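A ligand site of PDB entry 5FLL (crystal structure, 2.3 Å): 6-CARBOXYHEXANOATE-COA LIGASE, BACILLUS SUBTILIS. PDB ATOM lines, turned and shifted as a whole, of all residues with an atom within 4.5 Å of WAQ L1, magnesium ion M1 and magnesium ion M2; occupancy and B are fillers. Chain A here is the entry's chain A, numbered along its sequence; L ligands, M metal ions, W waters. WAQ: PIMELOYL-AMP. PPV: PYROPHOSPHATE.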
ATOM      1  N   HIS A  27     -13.118 -33.613 -28.912  1.00  0.00           N
ATOM      2  CA  HIS A  27     -13.699 -32.285 -28.774  1.00  0.00           C
ATOM      3  C   HIS A  27     -13.277 -31.714 -27.440  1.00  0.00           C
ATOM      4  O   HIS A  27     -13.324 -32.400 -26.410  1.00  0.00           O
ATOM      5  CB  HIS A  27     -15.215 -32.374 -28.831  1.00  0.00           C
ATOM      6  CG  HIS A  27     -15.904 -31.115 -28.451  1.00  0.00           C
ATOM      7  ND1 HIS A  27     -15.929 -30.013 -29.270  1.00  0.00           N
ATOM      8  CD2 HIS A  27     -16.627 -30.779 -27.347  1.00  0.00           C
ATOM      9  CE1 HIS A  27     -16.650 -29.050 -28.698  1.00  0.00           C
ATOM     10  NE2 HIS A  27     -17.103 -29.505 -27.540  1.00  0.00           N
ATOM     11  N   GLY A  30     -16.367 -25.647 -27.321  1.00  0.00           N
ATOM     12  CA  GLY A  30     -17.196 -25.001 -28.317  1.00  0.00           C
ATOM     13  C   GLY A  30     -17.771 -23.733 -27.735  1.00  0.00           C
ATOM     14  O   GLY A  30     -18.066 -23.652 -26.536  1.00  0.00           O
ATOM     15  N   GLU A  32     -20.385 -20.080 -28.815  1.00  0.00           N
ATOM     16  CA  GLU A  32     -21.227 -19.294 -29.700  1.00  0.00           C
ATOM     17  C   GLU A  32     -21.602 -17.962 -29.024  1.00  0.00           C
ATOM     18  O   GLU A  32     -21.929 -17.913 -27.829  1.00  0.00           O
ATOM     19  CB  GLU A  32     -22.481 -20.084 -30.088  1.00  0.00           C
ATOM     20  CG  GLU A  32     -23.036 -20.919 -28.947  1.00  0.00           C
ATOM     21  CD  GLU A  32     -22.424 -22.310 -28.901  1.00  0.00           C
ATOM     22  OE1 GLU A  32     -22.110 -22.877 -29.960  1.00  0.00           O
ATOM     23  OE2 GLU A  32     -22.284 -22.855 -27.785  1.00  0.00           O
ATOM     24  N   LYS A  50     -11.064 -19.234 -23.890  1.00  0.00           N
ATOM     25  CA  LYS A  50     -11.937 -20.323 -23.464  1.00  0.00           C
ATOM     26  C   LYS A  50     -11.467 -21.650 -24.020  1.00  0.00           C
ATOM     27  O   LYS A  50     -11.355 -22.626 -23.293  1.00  0.00           O
ATOM     28  CB  LYS A  50     -13.356 -20.047 -23.912  1.00  0.00           C
ATOM     29  CG  LYS A  50     -14.358 -21.169 -23.733  1.00  0.00           C
ATOM     30  CD  LYS A  50     -15.720 -20.704 -24.210  1.00  0.00           C
ATOM     31  CE  LYS A  50     -16.741 -21.833 -24.287  1.00  0.00           C
ATOM     32  NZ  LYS A  50     -17.352 -22.123 -22.952  1.00  0.00           N
ATOM     33  N   HIS A  54      -8.961 -25.010 -21.416  1.00  0.00           N
ATOM     34  CA  HIS A  54     -10.027 -25.923 -21.073  1.00  0.00           C
ATOM     35  C   HIS A  54      -9.515 -27.101 -20.257  1.00  0.00           C
ATOM     36  O   HIS A  54      -8.451 -27.633 -20.518  1.00  0.00           O
ATOM     37  CB  HIS A  54     -10.758 -26.425 -22.328  1.00  0.00           C
ATOM     38  CG  HIS A  54     -12.152 -26.873 -22.072  1.00  0.00           C
ATOM     39  ND1 HIS A  54     -12.443 -28.067 -21.452  1.00  0.00           N
ATOM     40  CD2 HIS A  54     -13.345 -26.272 -22.321  1.00  0.00           C
ATOM     41  CE1 HIS A  54     -13.757 -28.192 -21.336  1.00  0.00           C
ATOM     42  NE2 HIS A  54     -14.327 -27.117 -21.863  1.00  0.00           N
ATOM     43  N   VAL A 123     -20.967 -36.867 -28.362  1.00  0.00           N
ATOM     44  CA  VAL A 123     -21.619 -35.963 -29.277  1.00  0.00           C
ATOM     45  C   VAL A 123     -21.199 -34.535 -28.933  1.00  0.00           C
ATOM     46  O   VAL A 123     -21.152 -34.178 -27.771  1.00  0.00           O
ATOM     47  CB  VAL A 123     -23.144 -36.119 -29.209  1.00  0.00           C
ATOM     48  CG1 VAL A 123     -23.801 -35.029 -30.016  1.00  0.00           C
ATOM     49  CG2 VAL A 123     -23.535 -37.510 -29.720  1.00  0.00           C
ATOM     50  N   ARG A 124     -20.900 -33.752 -29.958  1.00  0.00           N
ATOM     51  CA  ARG A 124     -20.309 -32.414 -29.834  1.00  0.00           C
ATOM     52  C   ARG A 124     -21.337 -31.316 -29.696  1.00  0.00           C
ATOM     53  O   ARG A 124     -21.026 -30.209 -29.228  1.00  0.00           O
ATOM     54  CB  ARG A 124     -19.426 -32.167 -31.039  1.00  0.00           C
ATOM     55  CG  ARG A 124     -18.546 -33.374 -31.296  1.00  0.00           C
ATOM     56  CD  ARG A 124     -17.245 -33.032 -31.969  1.00  0.00           C
ATOM     57  NE  ARG A 124     -17.437 -32.766 -33.394  1.00  0.00           N
ATOM     58  CZ  ARG A 124     -17.587 -33.707 -34.322  1.00  0.00           C
ATOM     59  NH1 ARG A 124     -17.615 -34.998 -33.986  1.00  0.00           N
ATOM     60  NH2 ARG A 124     -17.746 -33.351 -35.590  1.00  0.00           N
ATOM     61  N   GLY A 125     -22.567 -31.613 -30.097  1.00  0.00           N
ATOM     62  CA  GLY A 125     -23.702 -30.733 -29.848  1.00  0.00           C
ATOM     63  C   GLY A 125     -24.772 -31.450 -29.029  1.00  0.00           C
ATOM     64  O   GLY A 125     -24.473 -32.156 -28.074  1.00  0.00           O
ATOM     65  N   ALA A 126     -26.040 -31.311 -29.461  1.00  0.00           N
ATOM     66  CA  ALA A 126     -27.159 -31.909 -28.740  1.00  0.00           C
ATOM     67  C   ALA A 126     -27.811 -33.008 -29.513  1.00  0.00           C
ATOM     68  O   ALA A 126     -27.756 -33.045 -30.737  1.00  0.00           O
ATOM     69  CB  ALA A 126     -28.194 -30.832 -28.417  1.00  0.00           C
ATOM     70  N   VAL A 145     -26.431 -31.536 -32.870  1.00  0.00           N
ATOM     71  CA  VAL A 145     -27.015 -30.295 -33.331  1.00  0.00           C
ATOM     72  C   VAL A 145     -26.481 -29.187 -32.436  1.00  0.00           C
ATOM     73  O   VAL A 145     -26.588 -29.266 -31.230  1.00  0.00           O
ATOM     74  CB  VAL A 145     -28.549 -30.341 -33.210  1.00  0.00           C
ATOM     75  CG1 VAL A 145     -29.155 -28.976 -33.499  1.00  0.00           C
ATOM     76  CG2 VAL A 145     -29.134 -31.372 -34.158  1.00  0.00           C
ATOM     77  N   ARG A 146     -25.900 -28.185 -33.041  1.00  0.00           N
ATOM     78  CA  ARG A 146     -25.283 -27.099 -32.308  1.00  0.00           C
ATOM     79  C   ARG A 146     -26.164 -25.860 -32.378  1.00  0.00           C
ATOM     80  O   ARG A 146     -26.292 -25.236 -33.409  1.00  0.00           O
ATOM     81  CB  ARG A 146     -23.887 -26.801 -32.847  1.00  0.00           C
ATOM     82  CG  ARG A 146     -23.042 -25.965 -31.891  1.00  0.00           C
ATOM     83  CD  ARG A 146     -22.447 -26.766 -30.738  1.00  0.00           C
ATOM     84  NE  ARG A 146     -21.851 -25.855 -29.737  1.00  0.00           N
ATOM     85  CZ  ARG A 146     -21.133 -26.220 -28.660  1.00  0.00           C
ATOM     86  NH1 ARG A 146     -20.905 -27.492 -28.387  1.00  0.00           N
ATOM     87  NH2 ARG A 146     -20.640 -25.285 -27.859  1.00  0.00           N
ATOM     88  N   VAL A 147     -26.793 -25.555 -31.252  1.00  0.00           N
ATOM     89  CA  VAL A 147     -27.590 -24.377 -31.125  1.00  0.00           C
ATOM     90  C   VAL A 147     -26.634 -23.208 -31.143  1.00  0.00           C
ATOM     91  O   VAL A 147     -25.670 -23.195 -30.383  1.00  0.00           O
ATOM     92  CB  VAL A 147     -28.311 -24.356 -29.761  1.00  0.00           C
ATOM     93  CG1 VAL A 147     -29.186 -23.118 -29.643  1.00  0.00           C
ATOM     94  CG2 VAL A 147     -29.124 -25.610 -29.554  1.00  0.00           C
ATOM     95  N   MET A 150     -27.183 -17.352 -29.974  1.00  0.00           N
ATOM     96  CA  MET A 150     -27.776 -16.818 -28.765  1.00  0.00           C
ATOM     97  C   MET A 150     -26.673 -16.246 -27.865  1.00  0.00           C
ATOM     98  O   MET A 150     -25.545 -16.743 -27.865  1.00  0.00           O
ATOM     99  CB  MET A 150     -28.539 -17.900 -28.027  1.00  0.00           C
ATOM    100  CG  MET A 150     -27.661 -18.998 -27.410  1.00  0.00           C
ATOM    101  SD  MET A 150     -27.070 -20.135 -28.666  1.00  0.00           S
ATOM    102  CE  MET A 150     -26.580 -21.504 -27.667  1.00  0.00           C
ATOM    103  N   ARG A 171     -20.274 -19.724 -17.395  1.00  0.00           N
ATOM    104  CA  ARG A 171     -20.813 -21.045 -17.647  1.00  0.00           C
ATOM    105  C   ARG A 171     -22.335 -21.084 -17.457  1.00  0.00           C
ATOM    106  O   ARG A 171     -23.065 -21.849 -18.091  1.00  0.00           O
ATOM    107  CB  ARG A 171     -20.130 -21.996 -16.685  1.00  0.00           C
ATOM    108  CG  ARG A 171     -20.132 -23.429 -17.118  1.00  0.00           C
ATOM    109  CD  ARG A 171     -19.862 -24.306 -15.931  1.00  0.00           C
ATOM    110  NE  ARG A 171     -18.451 -24.533 -15.685  1.00  0.00           N
ATOM    111  CZ  ARG A 171     -17.718 -25.450 -16.321  1.00  0.00           C
ATOM    112  NH1 ARG A 171     -18.281 -26.185 -17.289  1.00  0.00           N
ATOM    113  NH2 ARG A 171     -16.446 -25.636 -15.984  1.00  0.00           N
ATOM    114  N   ILE A 172     -22.823 -20.298 -16.509  1.00  0.00           N
ATOM    115  CA  ILE A 172     -24.241 -20.299 -16.222  1.00  0.00           C
ATOM    116  C   ILE A 172     -24.868 -19.401 -17.236  1.00  0.00           C
ATOM    117  O   ILE A 172     -25.934 -19.701 -17.785  1.00  0.00           O
ATOM    118  CB  ILE A 172     -24.502 -19.799 -14.790  1.00  0.00           C
ATOM    119  CG1 ILE A 172     -23.818 -20.750 -13.804  1.00  0.00           C
ATOM    120  CG2 ILE A 172     -25.984 -19.689 -14.535  1.00  0.00           C
ATOM    121  CD1 ILE A 172     -23.933 -20.326 -12.349  1.00  0.00           C
ATOM    122  N   GLU A 174     -23.977 -18.995 -20.205  1.00  0.00           N
ATOM    123  CA  GLU A 174     -24.039 -19.702 -21.471  1.00  0.00           C
ATOM    124  C   GLU A 174     -25.101 -20.784 -21.449  1.00  0.00           C
ATOM    125  O   GLU A 174     -25.924 -20.873 -22.374  1.00  0.00           O
ATOM    126  CB  GLU A 174     -22.662 -20.261 -21.831  1.00  0.00           C
ATOM    127  CG  GLU A 174     -21.674 -19.149 -22.146  1.00  0.00           C
ATOM    128  CD  GLU A 174     -20.223 -19.599 -22.202  1.00  0.00           C
ATOM    129  OE1 GLU A 174     -19.957 -20.808 -22.014  1.00  0.00           O
ATOM    130  OE2 GLU A 174     -19.346 -18.716 -22.389  1.00  0.00           O
ATOM    131  N   ALA A 175     -25.128 -21.556 -20.365  1.00  0.00           N
ATOM    132  CA  ALA A 175     -26.134 -22.611 -20.212  1.00  0.00           C
ATOM    133  C   ALA A 175     -27.543 -22.063 -20.227  1.00  0.00           C
ATOM    134  O   ALA A 175     -28.446 -22.673 -20.819  1.00  0.00           O
ATOM    135  CB  ALA A 175     -25.917 -23.383 -18.922  1.00  0.00           C
ATOM    136  N   LEU A 178     -28.712 -20.703 -23.586  1.00  0.00           N
ATOM    137  CA  LEU A 178     -29.084 -21.844 -24.449  1.00  0.00           C
ATOM    138  C   LEU A 178     -30.376 -22.466 -24.014  1.00  0.00           C
ATOM    139  O   LEU A 178     -31.270 -22.705 -24.811  1.00  0.00           O
ATOM    140  CB  LEU A 178     -27.956 -22.896 -24.463  1.00  0.00           C
ATOM    141  CG  LEU A 178     -28.205 -24.172 -25.276  1.00  0.00           C
ATOM    142  CD1 LEU A 178     -26.881 -24.892 -25.538  1.00  0.00           C
ATOM    143  CD2 LEU A 178     -29.122 -25.104 -24.534  1.00  0.00           C
ATOM    144  N   CYS A 193     -29.334 -31.835 -19.238  1.00  0.00           N
ATOM    145  CA  CYS A 193     -27.977 -31.365 -19.459  1.00  0.00           C
ATOM    146  C   CYS A 193     -27.051 -31.574 -18.256  1.00  0.00           C
ATOM    147  O   CYS A 193     -27.405 -31.244 -17.113  1.00  0.00           O
ATOM    148  CB  CYS A 193     -27.998 -29.878 -19.727  1.00  0.00           C
ATOM    149  SG  CYS A 193     -26.337 -29.169 -19.671  1.00  0.00           S
ATOM    150  N   TRP A 194     -25.868 -32.099 -18.528  1.00  0.00           N
ATOM    151  CA  TRP A 194     -24.748 -31.828 -17.667  1.00  0.00           C
ATOM    152  C   TRP A 194     -23.469 -31.761 -18.491  1.00  0.00           C
ATOM    153  O   TRP A 194     -23.413 -32.168 -19.657  1.00  0.00           O
ATOM    154  CB  TRP A 194     -24.672 -32.851 -16.520  1.00  0.00           C
ATOM    155  CG  TRP A 194     -24.431 -34.293 -16.889  1.00  0.00           C
ATOM    156  CD1 TRP A 194     -23.230 -34.907 -16.973  1.00  0.00           C
ATOM    157  CD2 TRP A 194     -25.407 -35.305 -17.136  1.00  0.00           C
ATOM    158  NE1 TRP A 194     -23.378 -36.226 -17.288  1.00  0.00           N
ATOM    159  CE2 TRP A 194     -24.711 -36.509 -17.376  1.00  0.00           C
ATOM    160  CE3 TRP A 194     -26.804 -35.316 -17.214  1.00  0.00           C
ATOM    161  CZ2 TRP A 194     -25.360 -37.698 -17.702  1.00  0.00           C
ATOM    162  CZ3 TRP A 194     -27.439 -36.485 -17.512  1.00  0.00           C
ATOM    163  CH2 TRP A 194     -26.722 -37.672 -17.735  1.00  0.00           C
ATOM    164  N   SER A 195     -22.423 -31.220 -17.872  1.00  0.00           N
ATOM    165  CA  SER A 195     -21.225 -30.869 -18.608  1.00  0.00           C
ATOM    166  C   SER A 195     -20.364 -32.081 -18.921  1.00  0.00           C
ATOM    167  O   SER A 195     -20.307 -33.046 -18.160  1.00  0.00           O
ATOM    168  CB  SER A 195     -20.417 -29.818 -17.828  1.00  0.00           C
ATOM    169  OG  SER A 195     -19.336 -29.358 -18.631  1.00  0.00           O
ATOM    170  N   ASP A 196     -19.675 -32.018 -20.057  1.00  0.00           N
ATOM    171  CA  ASP A 196     -18.614 -32.964 -20.368  1.00  0.00           C
ATOM    172  C   ASP A 196     -17.277 -32.561 -19.733  1.00  0.00           C
ATOM    173  O   ASP A 196     -16.262 -33.230 -19.952  1.00  0.00           O
ATOM    174  CB  ASP A 196     -18.472 -33.142 -21.889  1.00  0.00           C
ATOM    175  CG  ASP A 196     -18.112 -31.859 -22.606  1.00  0.00           C
ATOM    176  OD1 ASP A 196     -18.510 -30.769 -22.157  1.00  0.00           O
ATOM    177  OD2 ASP A 196     -17.411 -31.935 -23.652  1.00  0.00           O
ATOM    178  N   ASP A 197     -17.256 -31.469 -18.955  1.00  0.00           N
ATOM    179  CA  ASP A 197     -15.967 -31.025 -18.375  1.00  0.00           C
ATOM    180  C   ASP A 197     -15.659 -31.790 -17.087  1.00  0.00           C
ATOM    181  O   ASP A 197     -16.530 -32.001 -16.266  1.00  0.00           O
ATOM    182  CB  ASP A 197     -15.978 -29.518 -18.103  1.00  0.00           C
ATOM    183  CG  ASP A 197     -16.476 -28.686 -19.290  1.00  0.00           C
ATOM    184  OD1 ASP A 197     -16.646 -29.181 -20.424  1.00  0.00           O
ATOM    185  OD2 ASP A 197     -16.741 -27.499 -19.058  1.00  0.00           O
ATOM    186  N   TYR A 200     -16.703 -29.740 -13.527  1.00  0.00           N
ATOM    187  CA  TYR A 200     -17.986 -29.137 -13.180  1.00  0.00           C
ATOM    188  C   TYR A 200     -19.062 -30.191 -13.152  1.00  0.00           C
ATOM    189  O   TYR A 200     -19.358 -30.771 -14.196  1.00  0.00           O
ATOM    190  CB  TYR A 200     -18.348 -28.072 -14.200  1.00  0.00           C
ATOM    191  CG  TYR A 200     -19.360 -27.085 -13.701  1.00  0.00           C
ATOM    192  CD1 TYR A 200     -19.007 -26.115 -12.753  1.00  0.00           C
ATOM    193  CD2 TYR A 200     -20.670 -27.132 -14.138  1.00  0.00           C
ATOM    194  CE1 TYR A 200     -19.947 -25.204 -12.271  1.00  0.00           C
ATOM    195  CE2 TYR A 200     -21.620 -26.229 -13.677  1.00  0.00           C
ATOM    196  CZ  TYR A 200     -21.258 -25.275 -12.737  1.00  0.00           C
ATOM    197  OH  TYR A 200     -22.208 -24.396 -12.280  1.00  0.00           O
ATOM    198  N   THR A 202     -22.325 -29.683 -11.706  1.00  0.00           N
ATOM    199  CA  THR A 202     -23.676 -29.189 -11.725  1.00  0.00           C
ATOM    200  C   THR A 202     -24.269 -29.296 -13.106  1.00  0.00           C
ATOM    201  O   THR A 202     -23.570 -29.119 -14.108  1.00  0.00           O
ATOM    202  CB  THR A 202     -23.769 -27.759 -11.237  1.00  0.00           C
ATOM    203  OG1 THR A 202     -23.507 -27.745  -9.821  1.00  0.00           O
ATOM    204  CG2 THR A 202     -25.149 -27.209 -11.494  1.00  0.00           C
ATOM    205  N   GLY A 203     -25.543 -29.683 -13.158  1.00  0.00           N
ATOM    206  CA  GLY A 203     -26.273 -29.817 -14.422  1.00  0.00           C
ATOM    207  C   GLY A 203     -27.660 -29.220 -14.248  1.00  0.00           C
ATOM    208  O   GLY A 203     -27.921 -28.517 -13.268  1.00  0.00           O
ATOM    209  N   TYR A 204     -28.558 -29.503 -15.202  1.00  0.00           N
ATOM    210  CA  TYR A 204     -29.934 -29.004 -15.122  1.00  0.00           C
ATOM    211  C   TYR A 204     -30.918 -29.752 -15.977  1.00  0.00           C
ATOM    212  O   TYR A 204     -30.539 -30.511 -16.889  1.00  0.00           O
ATOM    213  CB  TYR A 204     -29.992 -27.528 -15.503  1.00  0.00           C
ATOM    214  CG  TYR A 204     -29.755 -27.210 -16.987  1.00  0.00           C
ATOM    215  CD1 TYR A 204     -30.814 -27.179 -17.881  1.00  0.00           C
ATOM    216  CD2 TYR A 204     -28.476 -26.866 -17.463  1.00  0.00           C
ATOM    217  CE1 TYR A 204     -30.622 -26.857 -19.196  1.00  0.00           C
ATOM    218  CE2 TYR A 204     -28.278 -26.570 -18.795  1.00  0.00           C
ATOM    219  CZ  TYR A 204     -29.340 -26.557 -19.641  1.00  0.00           C
ATOM    220  OH  TYR A 204     -29.143 -26.267 -20.965  1.00  0.00           O
ATOM    221  N   TYR A 212     -35.784 -23.374 -15.414  1.00  0.00           N
ATOM    222  CA  TYR A 212     -34.406 -23.850 -15.440  1.00  0.00           C
ATOM    223  C   TYR A 212     -34.093 -24.413 -14.056  1.00  0.00           C
ATOM    224  O   TYR A 212     -33.902 -23.660 -13.106  1.00  0.00           O
ATOM    225  CB  TYR A 212     -33.473 -22.674 -15.743  1.00  0.00           C
ATOM    226  CG  TYR A 212     -31.995 -22.979 -15.877  1.00  0.00           C
ATOM    227  CD1 TYR A 212     -31.480 -23.582 -17.012  1.00  0.00           C
ATOM    228  CD2 TYR A 212     -31.097 -22.576 -14.899  1.00  0.00           C
ATOM    229  CE1 TYR A 212     -30.128 -23.860 -17.151  1.00  0.00           C
ATOM    230  CE2 TYR A 212     -29.744 -22.783 -15.023  1.00  0.00           C
ATOM    231  CZ  TYR A 212     -29.258 -23.456 -16.139  1.00  0.00           C
ATOM    232  OH  TYR A 212     -27.910 -23.655 -16.259  1.00  0.00           O
ATOM    233  N   ARG A 214     -31.789 -26.200 -11.729  1.00  0.00           N
ATOM    234  CA  ARG A 214     -30.422 -26.594 -11.524  1.00  0.00           C
ATOM    235  C   ARG A 214     -30.361 -27.699 -10.502  1.00  0.00           C
ATOM    236  O   ARG A 214     -31.177 -27.767  -9.567  1.00  0.00           O
ATOM    237  CB  ARG A 214     -29.618 -25.402 -11.030  1.00  0.00           C
ATOM    238  CG  ARG A 214     -29.631 -24.240 -12.003  1.00  0.00           C
ATOM    239  CD  ARG A 214     -28.995 -23.005 -11.409  1.00  0.00           C
ATOM    240  NE  ARG A 214     -27.547 -23.080 -11.445  1.00  0.00           N
ATOM    241  CZ  ARG A 214     -26.774 -23.052 -10.362  1.00  0.00           C
ATOM    242  NH1 ARG A 214     -27.304 -22.965  -9.164  1.00  0.00           N
ATOM    243  NH2 ARG A 214     -25.462 -23.100 -10.504  1.00  0.00           N
ATOM    244  N   CYS A 227     -23.984 -34.707 -21.139  1.00  0.00           N
ATOM    245  CA  CYS A 227     -25.269 -34.994 -21.731  1.00  0.00           C
ATOM    246  C   CYS A 227     -25.945 -33.712 -22.205  1.00  0.00           C
ATOM    247  O   CYS A 227     -26.026 -32.732 -21.465  1.00  0.00           O
ATOM    248  CB  CYS A 227     -26.166 -35.696 -20.720  1.00  0.00           C
ATOM    249  SG  CYS A 227     -27.853 -36.042 -21.279  1.00  0.00           S
ATOM    250  N   ARG A 228     -26.471 -33.741 -23.417  1.00  0.00           N
ATOM    251  CA  ARG A 228     -27.344 -32.671 -23.892  1.00  0.00           C
ATOM    252  C   ARG A 228     -28.384 -33.303 -24.800  1.00  0.00           C
ATOM    253  O   ARG A 228     -28.108 -33.621 -25.961  1.00  0.00           O
ATOM    254  CB  ARG A 228     -26.531 -31.615 -24.665  1.00  0.00           C
ATOM    255  CG  ARG A 228     -26.996 -30.178 -24.514  1.00  0.00           C
ATOM    256  CD  ARG A 228     -26.818 -29.764 -23.076  1.00  0.00           C
ATOM    257  NE  ARG A 228     -27.115 -28.376 -22.768  1.00  0.00           N
ATOM    258  CZ  ARG A 228     -26.189 -27.450 -22.567  1.00  0.00           C
ATOM    259  NH1 ARG A 228     -24.895 -27.722 -22.761  1.00  0.00           N
ATOM    260  NH2 ARG A 228     -26.561 -26.246 -22.169  1.00  0.00           N
HETATM  261  N1  WAQ L   1     -25.725 -26.578 -28.840  1.00  0.00           N
HETATM  262  C2  WAQ L   1     -26.009 -27.938 -28.675  1.00  0.00           C
HETATM  263  N3  WAQ L   1     -25.344 -28.660 -27.689  1.00  0.00           N
HETATM  264  C4  WAQ L   1     -24.420 -28.025 -26.938  1.00  0.00           C
HETATM  265  C5  WAQ L   1     -24.170 -26.708 -27.092  1.00  0.00           C
HETATM  266  C6  WAQ L   1     -24.805 -26.009 -28.050  1.00  0.00           C
HETATM  267  N6  WAQ L   1     -24.506 -24.726 -28.181  1.00  0.00           N
HETATM  268  N7  WAQ L   1     -23.239 -26.356 -26.194  1.00  0.00           N
HETATM  269  C8  WAQ L   1     -22.910 -27.422 -25.480  1.00  0.00           C
HETATM  270  N9  WAQ L   1     -23.651 -28.459 -25.938  1.00  0.00           N
HETATM  271  C1' WAQ L   1     -23.619 -29.855 -25.516  1.00  0.00           C
HETATM  272  C2' WAQ L   1     -22.321 -30.441 -26.010  1.00  0.00           C
HETATM  273  O2' WAQ L   1     -22.456 -31.826 -26.221  1.00  0.00           O
HETATM  274  C3' WAQ L   1     -21.397 -30.245 -24.815  1.00  0.00           C
HETATM  275  O3' WAQ L   1     -20.264 -31.104 -24.875  1.00  0.00           O
HETATM  276  C4' WAQ L   1     -22.332 -30.648 -23.720  1.00  0.00           C
HETATM  277  O4' WAQ L   1     -23.614 -30.077 -24.106  1.00  0.00           O
HETATM  278  C5' WAQ L   1     -21.917 -29.978 -22.403  1.00  0.00           C
HETATM  279  O5' WAQ L   1     -21.513 -28.711 -22.750  1.00  0.00           O
HETATM  280  OAB WAQ L   1     -24.498 -24.106 -13.004  1.00  0.00           O
HETATM  281  OAC WAQ L   1     -21.283 -26.285 -18.872  1.00  0.00           O
HETATM  282  OAD WAQ L   1     -19.637 -28.324 -20.993  1.00  0.00           O
HETATM  283  OAE WAQ L   1     -26.495 -23.377 -13.844  1.00  0.00           O
HETATM  284  OAH WAQ L   1     -20.852 -26.305 -22.157  1.00  0.00           O
HETATM  285  CAK WAQ L   1     -25.007 -26.547 -16.695  1.00  0.00           C
HETATM  286  CAL WAQ L   1     -25.078 -25.930 -15.268  1.00  0.00           C
HETATM  287  CAM WAQ L   1     -23.589 -26.516 -17.234  1.00  0.00           C
HETATM  288  CAN WAQ L   1     -24.902 -24.430 -15.316  1.00  0.00           C
HETATM  289  CAO WAQ L   1     -23.460 -27.403 -18.458  1.00  0.00           C
HETATM  290  OAU WAQ L   1     -22.115 -27.782 -20.437  1.00  0.00           O
HETATM  291  CAW WAQ L   1     -25.341 -23.946 -13.941  1.00  0.00           C
HETATM  292  CAX WAQ L   1     -22.171 -27.060 -19.282  1.00  0.00           C
HETATM  293  PBG WAQ L   1     -21.016 -27.682 -21.583  1.00  0.00           P
HETATM  294  O11 PPV L   2     -18.731 -27.759 -26.348  1.00  0.00           O
HETATM  295  P1  PPV L   2     -18.950 -27.235 -24.953  1.00  0.00           P
HETATM  296  O21 PPV L   2     -20.004 -26.172 -24.831  1.00  0.00           O
HETATM  297  O31 PPV L   2     -19.005 -28.295 -23.845  1.00  0.00           O
HETATM  298  OPP PPV L   2     -17.597 -26.351 -24.679  1.00  0.00           O
HETATM  299  P2  PPV L   2     -17.258 -25.703 -23.230  1.00  0.00           P
HETATM  300  O12 PPV L   2     -18.436 -24.831 -22.857  1.00  0.00           O
HETATM  301  O22 PPV L   2     -16.005 -24.892 -23.462  1.00  0.00           O
HETATM  302  O32 PPV L   2     -17.136 -26.910 -22.306  1.00  0.00           O
HETATM  303 MG    MG M   1     -20.360 -24.637 -23.507  1.00  0.00          MG
HETATM  304 MG    MG M   2     -17.785 -28.746 -22.064  1.00  0.00          MG
HETATM  305  O   HOH W   1     -18.482 -25.391 -19.993  1.00  0.00           O
HETATM  306  O   HOH W   2     -16.359 -29.451 -23.541  1.00  0.00           O
HETATM  307  O   HOH W   3     -18.334 -33.909 -25.328  1.00  0.00           O
HETATM  308  O   HOH W   4     -22.329 -23.873 -19.722  1.00  0.00           O
HETATM  309  O   HOH W   5     -22.543 -24.459 -24.192  1.00  0.00           O
HETATM  310  O   HOH W   6     -20.866 -23.297 -22.002  1.00  0.00           O
HETATM  311  O   HOH W   7     -23.813 -24.811 -21.939  1.00  0.00           O
HETATM  312  O   HOH W   8     -19.964 -23.050 -24.759  1.00  0.00           O
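OG of Ser 195 lies within hydrogen-bond range of N of Asp 197 (3.0 Å). N of Cys 227 sits at hydrogen-bond distance from O of Trp 194 (3.0 Å). OD2 of Asp 197 lies within salt-bridge range of NH1 of Arg 171. The side-chain carboxylate of Asp 197 lies close to a ring nitrogen (NE2) of His 54, at 3.4 Å. NH2 of Arg 228 sits at hydrogen-bond distance from OH of Tyr 204. The backbone NH (N) of Tyr 204 is in hydrogen-bond range of the backbone carbonyl oxygen (O) of Cys 193, 2.8 Å away. NZ of Lys 50 is in salt-bridge range of OE1 of Glu 174, at 3.1 Å. NH2 of Arg 146 sits close to O of Gly 30, 3.3 Å away.
Magnesium ion M1 is bound by an oxygen (O12) of PPV L2 (2.0 Å), an oxygen (O21) of PPV L2 (2.1 Å), water W8 (2.1 Å), water W6 (2.1 Å), an oxygen (OAH) of WAQ L1 (2.2 Å) and water W5 (2.3 Å).
The guanidinium group (NH2) of Arg 146 sits close to a nitrogen (N7) of WAQ L1, at 3.3 Å. The backbone NH (N) of Gly 30 is in hydrogen-bond range of an oxygen (OPP) of PPV L2, at 3.0 Å. The backbone carbonyl oxygen (O) of Val 147 sits at hydrogen-bond distance from a nitrogen (N6) of WAQ L1 (2.9 Å). O4' of WAQ L1 lies within hydrogen-bond range of NH1 of Arg 228. The guanidinium group (NH1) of Arg 171 sits at hydrogen-bond distance from an oxygen (OAC) of WAQ L1 (3.4 Å). A ring nitrogen (NE2) of His 54 sits close to an oxygen (O22) of PPV L2 (3.2 Å). The side-chain carboxylate (OE2) of Glu 32 lies within hydrogen-bond range of a nitrogen (N6) of WAQ L1 (2.9 Å). NE2 of His 27 lies within hydrogen-bond range of O11 of PPV L2 (2.7 Å). N1 of WAQ L1 is in hydrogen-bond range of N of Val 147, at 2.8 Å. The backbone carbonyl oxygen (O) of Gly 125 sits at hydrogen-bond distance from an oxygen (O2') of WAQ L1 (2.8 Å). N of Ala 126 lies within hydrogen-bond range of N3 of WAQ L1 (3.3 Å). An oxygen (O22) of PPV L2 lies within salt-bridge range of the side-chain amino group of Lys 50, 3.1 Å away. O11 of PPV L2 is in salt-bridge range of NH1 of Arg 146 (3.0 Å). The guanidinium group (NE) of Arg 214 is in salt-bridge range of an oxygen (OAE) of WAQ L1 (2.6 Å). OH of Tyr 212 sits at hydrogen-bond distance from OAE of WAQ L1 (2.8 Å). The side-chain hydroxyl (OH) of Tyr 200 is in hydrogen-bond range of an oxygen (OAB) of WAQ L1 (2.4 Å). The backbone carbonyl oxygen (O) of Val 123 sits at hydrogen-bond distance from an oxygen (O2') of WAQ L1, at 3.1 Å. OG of Ser 195 lies close to OAD of WAQ L1, 2.6 Å away.
Gly 30 touches magnesium ion M1. Lys 50 touches magnesium ion M1.
Residues that only touch WAQ L1: Val 145, Leu 178, Arg 124, Thr 202, Ile 172, Tyr 204, Cys 193, Trp 194, Met 150 and Ala 175. Of the 31 residues printed, 24 come within 4 Å of WAQ L1.
NE2 of His 54 touches magnesium ion M2, 3.8 Å away. Ser 195 touches magnesium ion M2 (OG to MG, 3.8 Å). Four residues have an atom within 4 Å of magnesium ion M2: His 54, Ser 195, Asp 196 and Asp 197. The nearest printed residue that does not touch magnesium ion M2 is Arg 171 (5.4 Å).
An oxygen (O32) of PPV L2 binds magnesium ion M2. OD1 of Asp 197 is bound to magnesium ion M2. The side-chain carboxylate (OD1) of Asp 196 binds magnesium ion M2, 2.2 Å away. Water W2 is bound to magnesium ion M2 (2.2 Å). Magnesium ion M2 is bound by OAD of WAQ L1 (2.2 Å). Magnesium ion M2 is bound by O31 of PPV L2, 2.2 Å away. Magnesium ion M2 has six donor atoms within binding distance.
Water W8 bridges the backbone carbonyl oxygen of Gly 30 and the side-chain amino group of Lys 50. Water W4 bridges O of Arg 171 and OAC of WAQ L1. Water W1 lies within hydrogen-bond range of NH1 of Arg 171 (2.8 Å), OD2 of Asp 197 (2.9 Å) and OAC of WAQ L1 (3.1 Å). Water W3 lies within hydrogen-bond range of OD2 of Asp 196 and O3' of WAQ L1.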
